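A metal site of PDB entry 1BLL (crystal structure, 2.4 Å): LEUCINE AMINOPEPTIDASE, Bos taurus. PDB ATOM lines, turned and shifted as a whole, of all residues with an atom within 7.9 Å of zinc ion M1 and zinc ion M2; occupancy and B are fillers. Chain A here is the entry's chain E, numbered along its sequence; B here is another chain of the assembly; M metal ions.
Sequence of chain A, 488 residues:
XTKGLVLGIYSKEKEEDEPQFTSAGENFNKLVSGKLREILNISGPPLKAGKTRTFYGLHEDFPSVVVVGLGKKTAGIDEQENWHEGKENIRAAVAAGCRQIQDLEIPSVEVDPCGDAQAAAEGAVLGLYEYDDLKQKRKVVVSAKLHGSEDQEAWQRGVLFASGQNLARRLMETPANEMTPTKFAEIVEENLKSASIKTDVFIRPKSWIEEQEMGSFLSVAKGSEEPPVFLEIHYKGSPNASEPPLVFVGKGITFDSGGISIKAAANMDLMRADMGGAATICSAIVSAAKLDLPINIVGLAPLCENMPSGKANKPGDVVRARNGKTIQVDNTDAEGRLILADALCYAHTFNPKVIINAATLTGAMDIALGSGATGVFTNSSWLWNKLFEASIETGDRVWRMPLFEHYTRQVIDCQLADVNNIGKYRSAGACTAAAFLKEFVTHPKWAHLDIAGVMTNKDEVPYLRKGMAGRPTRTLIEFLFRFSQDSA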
ATOM      1  N   VAL A 220       8.755  29.184   3.332  1.00  0.00           N
ATOM      2  CA  VAL A 220       8.672  28.036   2.439  1.00  0.00           C
ATOM      3  C   VAL A 220       8.409  26.761   3.215  1.00  0.00           C
ATOM      4  O   VAL A 220       7.533  26.000   2.798  1.00  0.00           O
ATOM      5  CB  VAL A 220       9.960  27.838   1.655  1.00  0.00           C
ATOM      6  CG1 VAL A 220       9.755  26.688   0.673  1.00  0.00           C
ATOM      7  CG2 VAL A 220      10.298  29.067   0.822  1.00  0.00           C
ATOM      8  N   LYS A 251      20.938  24.712  -2.012  1.00  0.00           N
ATOM      9  CA  LYS A 251      19.503  24.571  -1.878  1.00  0.00           C
ATOM     10  C   LYS A 251      19.139  23.154  -1.459  1.00  0.00           C
ATOM     11  O   LYS A 251      19.542  22.191  -2.106  1.00  0.00           O
ATOM     12  CB  LYS A 251      18.853  24.918  -3.229  1.00  0.00           C
ATOM     13  CG  LYS A 251      17.450  24.368  -3.353  1.00  0.00           C
ATOM     14  CD  LYS A 251      16.457  25.223  -4.049  1.00  0.00           C
ATOM     15  CE  LYS A 251      16.388  24.915  -5.502  1.00  0.00           C
ATOM     16  NZ  LYS A 251      15.019  24.558  -5.866  1.00  0.00           N
ATOM     17  N   ILE A 253      15.750  21.667  -0.988  1.00  0.00           N
ATOM     18  CA  ILE A 253      14.306  21.413  -0.977  1.00  0.00           C
ATOM     19  C   ILE A 253      14.185  19.896  -1.116  1.00  0.00           C
ATOM     20  O   ILE A 253      14.585  19.397  -2.174  1.00  0.00           O
ATOM     21  CB  ILE A 253      13.607  22.205  -2.147  1.00  0.00           C
ATOM     22  CG1 ILE A 253      13.695  23.722  -1.907  1.00  0.00           C
ATOM     23  CG2 ILE A 253      12.168  21.788  -2.245  1.00  0.00           C
ATOM     24  CD1 ILE A 253      13.062  24.147  -0.573  1.00  0.00           C
ATOM     25  N   PHE A 255      11.647  17.946  -1.412  1.00  0.00           N
ATOM     26  CA  PHE A 255      10.709  17.724  -2.482  1.00  0.00           C
ATOM     27  C   PHE A 255      10.095  19.081  -2.844  1.00  0.00           C
ATOM     28  O   PHE A 255       9.665  19.822  -1.970  1.00  0.00           O
ATOM     29  CB  PHE A 255       9.638  16.709  -2.048  1.00  0.00           C
ATOM     30  CG  PHE A 255       8.787  16.325  -3.228  1.00  0.00           C
ATOM     31  CD1 PHE A 255       9.309  15.519  -4.231  1.00  0.00           C
ATOM     32  CD2 PHE A 255       7.547  16.950  -3.403  1.00  0.00           C
ATOM     33  CE1 PHE A 255       8.666  15.404  -5.443  1.00  0.00           C
ATOM     34  CE2 PHE A 255       6.894  16.833  -4.625  1.00  0.00           C
ATOM     35  CZ  PHE A 255       7.476  16.076  -5.644  1.00  0.00           C
ATOM     36  N   ASP A 256      10.110  19.454  -4.141  1.00  0.00           N
ATOM     37  CA  ASP A 256       9.475  20.664  -4.631  1.00  0.00           C
ATOM     38  C   ASP A 256       8.179  20.330  -5.386  1.00  0.00           C
ATOM     39  O   ASP A 256       8.175  19.953  -6.545  1.00  0.00           O
ATOM     40  CB  ASP A 256      10.462  21.442  -5.552  1.00  0.00           C
ATOM     41  CG  ASP A 256      10.052  22.857  -6.032  1.00  0.00           C
ATOM     42  OD1 ASP A 256       9.019  23.319  -5.493  1.00  0.00           O
ATOM     43  OD2 ASP A 256      10.752  23.467  -6.888  1.00  0.00           O
ATOM     44  N   SER A 257       7.008  20.411  -4.757  1.00  0.00           N
ATOM     45  CA  SER A 257       5.725  20.260  -5.442  1.00  0.00           C
ATOM     46  C   SER A 257       5.263  21.597  -6.000  1.00  0.00           C
ATOM     47  O   SER A 257       4.262  21.670  -6.703  1.00  0.00           O
ATOM     48  CB  SER A 257       4.625  19.782  -4.495  1.00  0.00           C
ATOM     49  OG  SER A 257       4.193  20.804  -3.619  1.00  0.00           O
ATOM     50  N   GLY A 258       5.949  22.690  -5.654  1.00  0.00           N
ATOM     51  CA  GLY A 258       5.566  23.999  -6.066  1.00  0.00           C
ATOM     52  C   GLY A 258       4.778  24.673  -4.983  1.00  0.00           C
ATOM     53  O   GLY A 258       4.823  25.894  -4.897  1.00  0.00           O
ATOM     54  N   GLY A 259       4.041  23.929  -4.141  1.00  0.00           N
ATOM     55  CA  GLY A 259       3.193  24.519  -3.108  1.00  0.00           C
ATOM     56  C   GLY A 259       1.879  24.944  -3.707  1.00  0.00           C
ATOM     57  O   GLY A 259       1.319  24.220  -4.515  1.00  0.00           O
ATOM     58  N   SER A 261       1.500  27.350  -5.836  1.00  0.00           N
ATOM     59  CA  SER A 261       1.751  27.511  -7.271  1.00  0.00           C
ATOM     60  C   SER A 261       2.237  26.143  -7.733  1.00  0.00           C
ATOM     61  O   SER A 261       3.386  25.940  -8.174  1.00  0.00           O
ATOM     62  CB  SER A 261       2.824  28.548  -7.531  1.00  0.00           C
ATOM     63  OG  SER A 261       2.408  29.803  -7.002  1.00  0.00           O
ATOM     64  N   LYS A 263       2.789  22.376  -9.100  1.00  0.00           N
ATOM     65  CA  LYS A 263       3.339  21.786 -10.291  1.00  0.00           C
ATOM     66  C   LYS A 263       2.424  20.799 -10.993  1.00  0.00           C
ATOM     67  O   LYS A 263       1.566  20.175 -10.388  1.00  0.00           O
ATOM     68  CB  LYS A 263       4.629  21.044  -9.979  1.00  0.00           C
ATOM     69  CG  LYS A 263       5.787  21.923  -9.663  1.00  0.00           C
ATOM     70  CD  LYS A 263       6.967  21.013  -9.409  1.00  0.00           C
ATOM     71  CE  LYS A 263       8.150  21.871  -9.036  1.00  0.00           C
ATOM     72  NZ  LYS A 263       8.440  22.830 -10.080  1.00  0.00           N
ATOM     73  N   MET A 271      11.560  15.977  -8.708  1.00  0.00           N
ATOM     74  CA  MET A 271      11.711  17.015  -7.697  1.00  0.00           C
ATOM     75  C   MET A 271      12.207  16.544  -6.348  1.00  0.00           C
ATOM     76  O   MET A 271      12.534  17.401  -5.531  1.00  0.00           O
ATOM     77  CB  MET A 271      10.410  17.760  -7.435  1.00  0.00           C
ATOM     78  CG  MET A 271       9.901  18.543  -8.629  1.00  0.00           C
ATOM     79  SD  MET A 271      11.214  19.272  -9.621  1.00  0.00           S
ATOM     80  CE  MET A 271      11.517  20.716  -8.707  1.00  0.00           C
ATOM     81  N   ALA A 273      14.953  15.436  -6.156  1.00  0.00           N
ATOM     82  CA  ALA A 273      16.343  15.863  -6.348  1.00  0.00           C
ATOM     83  C   ALA A 273      16.555  17.355  -6.324  1.00  0.00           C
ATOM     84  O   ALA A 273      17.595  17.832  -6.767  1.00  0.00           O
ATOM     85  CB  ALA A 273      16.863  15.396  -7.676  1.00  0.00           C
ATOM     86  N   ASP A 274      15.583  18.093  -5.775  1.00  0.00           N
ATOM     87  CA  ASP A 274      15.678  19.550  -5.633  1.00  0.00           C
ATOM     88  C   ASP A 274      16.483  19.988  -4.397  1.00  0.00           C
ATOM     89  O   ASP A 274      16.578  21.159  -4.035  1.00  0.00           O
ATOM     90  CB  ASP A 274      14.265  20.113  -5.581  1.00  0.00           C
ATOM     91  CG  ASP A 274      14.183  21.502  -6.158  1.00  0.00           C
ATOM     92  OD1 ASP A 274      14.762  21.728  -7.217  1.00  0.00           O
ATOM     93  OD2 ASP A 274      13.542  22.355  -5.571  1.00  0.00           O
ATOM     94  N   MET A 275      17.046  18.995  -3.690  1.00  0.00           N
ATOM     95  CA  MET A 275      18.080  19.207  -2.674  1.00  0.00           C
ATOM     96  C   MET A 275      19.471  18.919  -3.258  1.00  0.00           C
ATOM     97  O   MET A 275      20.436  18.746  -2.495  1.00  0.00           O
ATOM     98  CB  MET A 275      17.875  18.309  -1.434  1.00  0.00           C
ATOM     99  CG  MET A 275      17.349  16.879  -1.638  1.00  0.00           C
ATOM    100  SD  MET A 275      18.272  15.901  -2.837  1.00  0.00           S
ATOM    101  CE  MET A 275      19.627  15.717  -1.708  1.00  0.00           C
ATOM    102  N   ASN A 306       8.562  21.698  -0.034  1.00  0.00           N
ATOM    103  CA  ASN A 306       7.671  22.776  -0.434  1.00  0.00           C
ATOM    104  C   ASN A 306       6.311  22.195  -0.824  1.00  0.00           C
ATOM    105  O   ASN A 306       6.067  21.823  -1.949  1.00  0.00           O
ATOM    106  CB  ASN A 306       8.317  23.532  -1.596  1.00  0.00           C
ATOM    107  CG  ASN A 306       7.555  24.751  -2.103  1.00  0.00           C
ATOM    108  OD1 ASN A 306       7.550  24.963  -3.307  1.00  0.00           O
ATOM    109  ND2 ASN A 306       6.952  25.600  -1.295  1.00  0.00           N
ATOM    110  N   ASN A 331       5.073  33.799  -6.708  1.00  0.00           N
ATOM    111  CA  ASN A 331       4.978  32.440  -7.162  1.00  0.00           C
ATOM    112  C   ASN A 331       5.700  31.645  -6.093  1.00  0.00           C
ATOM    113  O   ASN A 331       6.864  31.876  -5.750  1.00  0.00           O
ATOM    114  CB  ASN A 331       5.661  32.290  -8.506  1.00  0.00           C
ATOM    115  CG  ASN A 331       5.479  30.917  -9.131  1.00  0.00           C
ATOM    116  OD1 ASN A 331       5.802  29.905  -8.555  1.00  0.00           O
ATOM    117  ND2 ASN A 331       4.939  30.808 -10.344  1.00  0.00           N
ATOM    118  N   THR A 332       4.914  30.718  -5.583  1.00  0.00           N
ATOM    119  CA  THR A 332       5.327  29.800  -4.525  1.00  0.00           C
ATOM    120  C   THR A 332       6.348  28.720  -4.981  1.00  0.00           C
ATOM    121  O   THR A 332       7.018  28.096  -4.155  1.00  0.00           O
ATOM    122  CB  THR A 332       3.988  29.278  -4.022  1.00  0.00           C
ATOM    123  OG1 THR A 332       3.427  30.366  -3.299  1.00  0.00           O
ATOM    124  CG2 THR A 332       4.053  28.125  -3.096  1.00  0.00           C
ATOM    125  N   ASP A 333       6.496  28.517  -6.295  1.00  0.00           N
ATOM    126  CA  ASP A 333       7.420  27.575  -6.906  1.00  0.00           C
ATOM    127  C   ASP A 333       8.754  28.224  -7.253  1.00  0.00           C
ATOM    128  O   ASP A 333       9.572  27.689  -8.018  1.00  0.00           O
ATOM    129  CB  ASP A 333       6.755  26.968  -8.153  1.00  0.00           C
ATOM    130  CG  ASP A 333       7.292  25.648  -8.731  1.00  0.00           C
ATOM    131  OD1 ASP A 333       8.062  24.931  -8.047  1.00  0.00           O
ATOM    132  OD2 ASP A 333       6.953  25.325  -9.880  1.00  0.00           O
ATOM    133  N   ALA A 334       8.987  29.410  -6.700  1.00  0.00           N
ATOM    134  CA  ALA A 334      10.300  30.045  -6.797  1.00  0.00           C
ATOM    135  C   ALA A 334      10.805  30.117  -5.346  1.00  0.00           C
ATOM    136  O   ALA A 334      10.994  31.196  -4.774  1.00  0.00           O
ATOM    137  CB  ALA A 334      10.145  31.439  -7.403  1.00  0.00           C
ATOM    138  N   GLU A 335      10.963  28.941  -4.726  1.00  0.00           N
ATOM    139  CA  GLU A 335      11.287  28.801  -3.307  1.00  0.00           C
ATOM    140  C   GLU A 335      12.734  28.634  -3.002  1.00  0.00           C
ATOM    141  O   GLU A 335      13.218  28.885  -1.894  1.00  0.00           O
ATOM    142  CB  GLU A 335      10.529  27.604  -2.646  1.00  0.00           C
ATOM    143  CG  GLU A 335      10.965  26.136  -2.817  1.00  0.00           C
ATOM    144  CD  GLU A 335      11.027  25.686  -4.267  1.00  0.00           C
ATOM    145  OE1 GLU A 335      10.075  25.999  -4.954  1.00  0.00           O
ATOM    146  OE2 GLU A 335      11.992  25.045  -4.684  1.00  0.00           O
ATOM    147  N   GLY A 336      13.471  28.188  -4.008  1.00  0.00           N
ATOM    148  CA  GLY A 336      14.915  28.081  -3.868  1.00  0.00           C
ATOM    149  C   GLY A 336      15.489  29.442  -3.582  1.00  0.00           C
ATOM    150  O   GLY A 336      16.223  29.578  -2.610  1.00  0.00           O
ATOM    151  N   ARG A 337      15.007  30.442  -4.339  1.00  0.00           N
ATOM    152  CA  ARG A 337      15.381  31.865  -4.244  1.00  0.00           C
ATOM    153  C   ARG A 337      15.303  32.301  -2.795  1.00  0.00           C
ATOM    154  O   ARG A 337      16.219  32.866  -2.220  1.00  0.00           O
ATOM    155  CB  ARG A 337      14.410  32.801  -5.042  1.00  0.00           C
ATOM    156  CG  ARG A 337      14.197  32.766  -6.582  1.00  0.00           C
ATOM    157  CD  ARG A 337      14.676  31.388  -7.066  1.00  0.00           C
ATOM    158  NE  ARG A 337      13.793  30.683  -7.969  1.00  0.00           N
ATOM    159  CZ  ARG A 337      13.472  29.396  -7.858  1.00  0.00           C
ATOM    160  NH1 ARG A 337      13.856  28.593  -6.876  1.00  0.00           N
ATOM    161  NH2 ARG A 337      12.676  28.947  -8.803  1.00  0.00           N
ATOM    162  N   ALA A 359      22.472  25.245  -6.914  1.00  0.00           N
ATOM    163  CA  ALA A 359      21.041  25.016  -6.820  1.00  0.00           C
ATOM    164  C   ALA A 359      20.355  24.561  -8.080  1.00  0.00           C
ATOM    165  O   ALA A 359      20.615  25.089  -9.151  1.00  0.00           O
ATOM    166  CB  ALA A 359      20.301  26.288  -6.385  1.00  0.00           C
ATOM    167  N   THR A 360      19.427  23.606  -7.923  1.00  0.00           N
ATOM    168  CA  THR A 360      18.552  23.153  -9.009  1.00  0.00           C
ATOM    169  C   THR A 360      17.435  24.199  -9.028  1.00  0.00           C
ATOM    170  O   THR A 360      16.298  24.007  -8.571  1.00  0.00           O
ATOM    171  CB  THR A 360      18.054  21.736  -8.639  1.00  0.00           C
ATOM    172  OG1 THR A 360      17.485  21.850  -7.350  1.00  0.00           O
ATOM    173  CG2 THR A 360      19.160  20.696  -8.609  1.00  0.00           C
ATOM    174  N   LEU A 361      17.811  25.380  -9.534  1.00  0.00           N
ATOM    175  CA  LEU A 361      16.985  26.569  -9.399  1.00  0.00           C
ATOM    176  C   LEU A 361      15.867  26.861 -10.368  1.00  0.00           C
ATOM    177  O   LEU A 361      14.795  27.284  -9.944  1.00  0.00           O
ATOM    178  CB  LEU A 361      17.882  27.822  -9.401  1.00  0.00           C
ATOM    179  CG  LEU A 361      17.968  28.826  -8.253  1.00  0.00           C
ATOM    180  CD1 LEU A 361      17.796  30.169  -8.905  1.00  0.00           C
ATOM    181  CD2 LEU A 361      17.006  28.520  -7.127  1.00  0.00           C
ATOM    182  N   THR A 362      16.126  26.748 -11.673  1.00  0.00           N
ATOM    183  CA  THR A 362      15.168  27.107 -12.676  1.00  0.00           C
ATOM    184  C   THR A 362      15.193  26.074 -13.769  1.00  0.00           C
ATOM    185  O   THR A 362      16.236  25.559 -14.102  1.00  0.00           O
ATOM    186  CB  THR A 362      15.492  28.530 -13.316  1.00  0.00           C
ATOM    187  OG1 THR A 362      16.608  28.397 -14.170  1.00  0.00           O
ATOM    188  CG2 THR A 362      15.851  29.603 -12.304  1.00  0.00           C
ATOM    189  N   L2O B   1      13.490  23.383  -8.353  1.00  0.00           N
ATOM    190  CA  L2O B   1      12.864  23.868  -9.578  1.00  0.00           C
ATOM    191  C2  L2O B   1      13.978  23.902 -10.525  1.00  0.00           C
ATOM    192  C3  L2O B   1      13.811  23.094 -11.761  1.00  0.00           C
ATOM    193  C4  L2O B   1      12.310  22.914 -11.983  1.00  0.00           C
ATOM    194  C5  L2O B   1      14.465  21.716 -11.573  1.00  0.00           C
ATOM    195  C6  L2O B   1      12.227  25.231  -9.336  1.00  0.00           C
ATOM    196  O1  L2O B   1      11.757  25.358  -8.017  1.00  0.00           O
ATOM    197  C   L2O B   1      11.079  25.447 -10.353  1.00  0.00           C
ATOM    198  O   L2O B   1      10.334  24.622 -10.809  1.00  0.00           O
ATOM    199  N   VAL B   2      10.999  26.741 -10.730  1.00  0.00           N
ATOM    200  CA  VAL B   2      10.022  27.239 -11.627  1.00  0.00           C
ATOM    201  C   VAL B   2      10.384  26.943 -13.095  1.00  0.00           C
ATOM    202  O   VAL B   2      11.537  26.678 -13.431  1.00  0.00           O
ATOM    203  CB  VAL B   2       9.798  28.767 -11.493  1.00  0.00           C
ATOM    204  CG1 VAL B   2      10.989  29.504 -12.120  1.00  0.00           C
ATOM    205  CG2 VAL B   2       8.509  29.221 -12.190  1.00  0.00           C
ATOM    206  N   VAL B   3       9.350  26.995 -13.961  1.00  0.00           N
ATOM    207  CA  VAL B   3       9.438  26.479 -15.328  1.00  0.00           C
ATOM    208  C   VAL B   3       9.685  27.559 -16.337  1.00  0.00           C
ATOM    209  O   VAL B   3       9.443  28.711 -15.963  1.00  0.00           O
ATOM    210  CB  VAL B   3       8.024  26.060 -15.709  1.00  0.00           C
ATOM    211  CG1 VAL B   3       7.392  25.181 -14.622  1.00  0.00           C
ATOM    212  CG2 VAL B   3       7.266  27.394 -15.760  1.00  0.00           C
HETATM  213 ZN    ZN M   1      12.849  24.198  -6.532  1.00  0.00          ZN
HETATM  214 ZN    ZN M   2       9.926  25.529  -7.088  1.00  0.00          ZN
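N of Val 2 of chain B sits close to O of Asp 333, 3.2 Å away. The side-chain carboxylate (OD2) of Asp 333 is in salt-bridge range of the side-chain amino group (NZ) of Lys 263 (2.9 Å). OE1 of Glu 335 sits close to OD1 of Asn 306 (3.2 Å). The backbone NH of Ile 253 is in hydrogen-bond range of the backbone carbonyl oxygen of Asp 274, 3.2 Å away. OD2 of Asp 256 sits close to NZ of Lys 263 (3.99 Å). N of Asp 256 is in hydrogen-bond range of O of Met 271 (3.5 Å). The side-chain carboxylate (OD1) of Asp 256 lies close to the side-chain amide oxygen (OD1) of Asn 306. NZ of Lys 251 sits close to O of Thr 360.
Along chain A the residues within 4 Å of zinc ion M1 span positions 251 to 335. The nearest printed residue that does not touch zinc ion M1 is Thr 360 (4.01 Å).
Residues that only touch zinc ion M2: Val 2 of chain B. Within 4 Å of zinc ion M2: Asp 256, Asp 333, Glu 335, L2O 1 of chain B and Val 2 of chain B. The nearest printed residue that does not touch zinc ion M2 is Ala 334 (4.01 Å).
Zinc ion M1 is bound by N of L2O 1 of chain B (2.1 Å), O1 of L2O 1 of chain B (2.2 Å), OD2 of Asp 274 (2.2 Å), OE2 of Glu 335 (2.2 Å), OD2 of Asp 256 (2.2 Å) and NZ of Lys 251 (2.3 Å). Zinc ion M1 has six donor atoms within binding distance.
Zinc ion M2 is bound by O1 of L2O 1 of chain B (2.1 Å), OD1 of Asp 333 (2.2 Å), OE1 of Glu 335 (2.2 Å), OD2 of Asp 256 (2.2 Å) and O of Asp 333 (2.4 Å).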
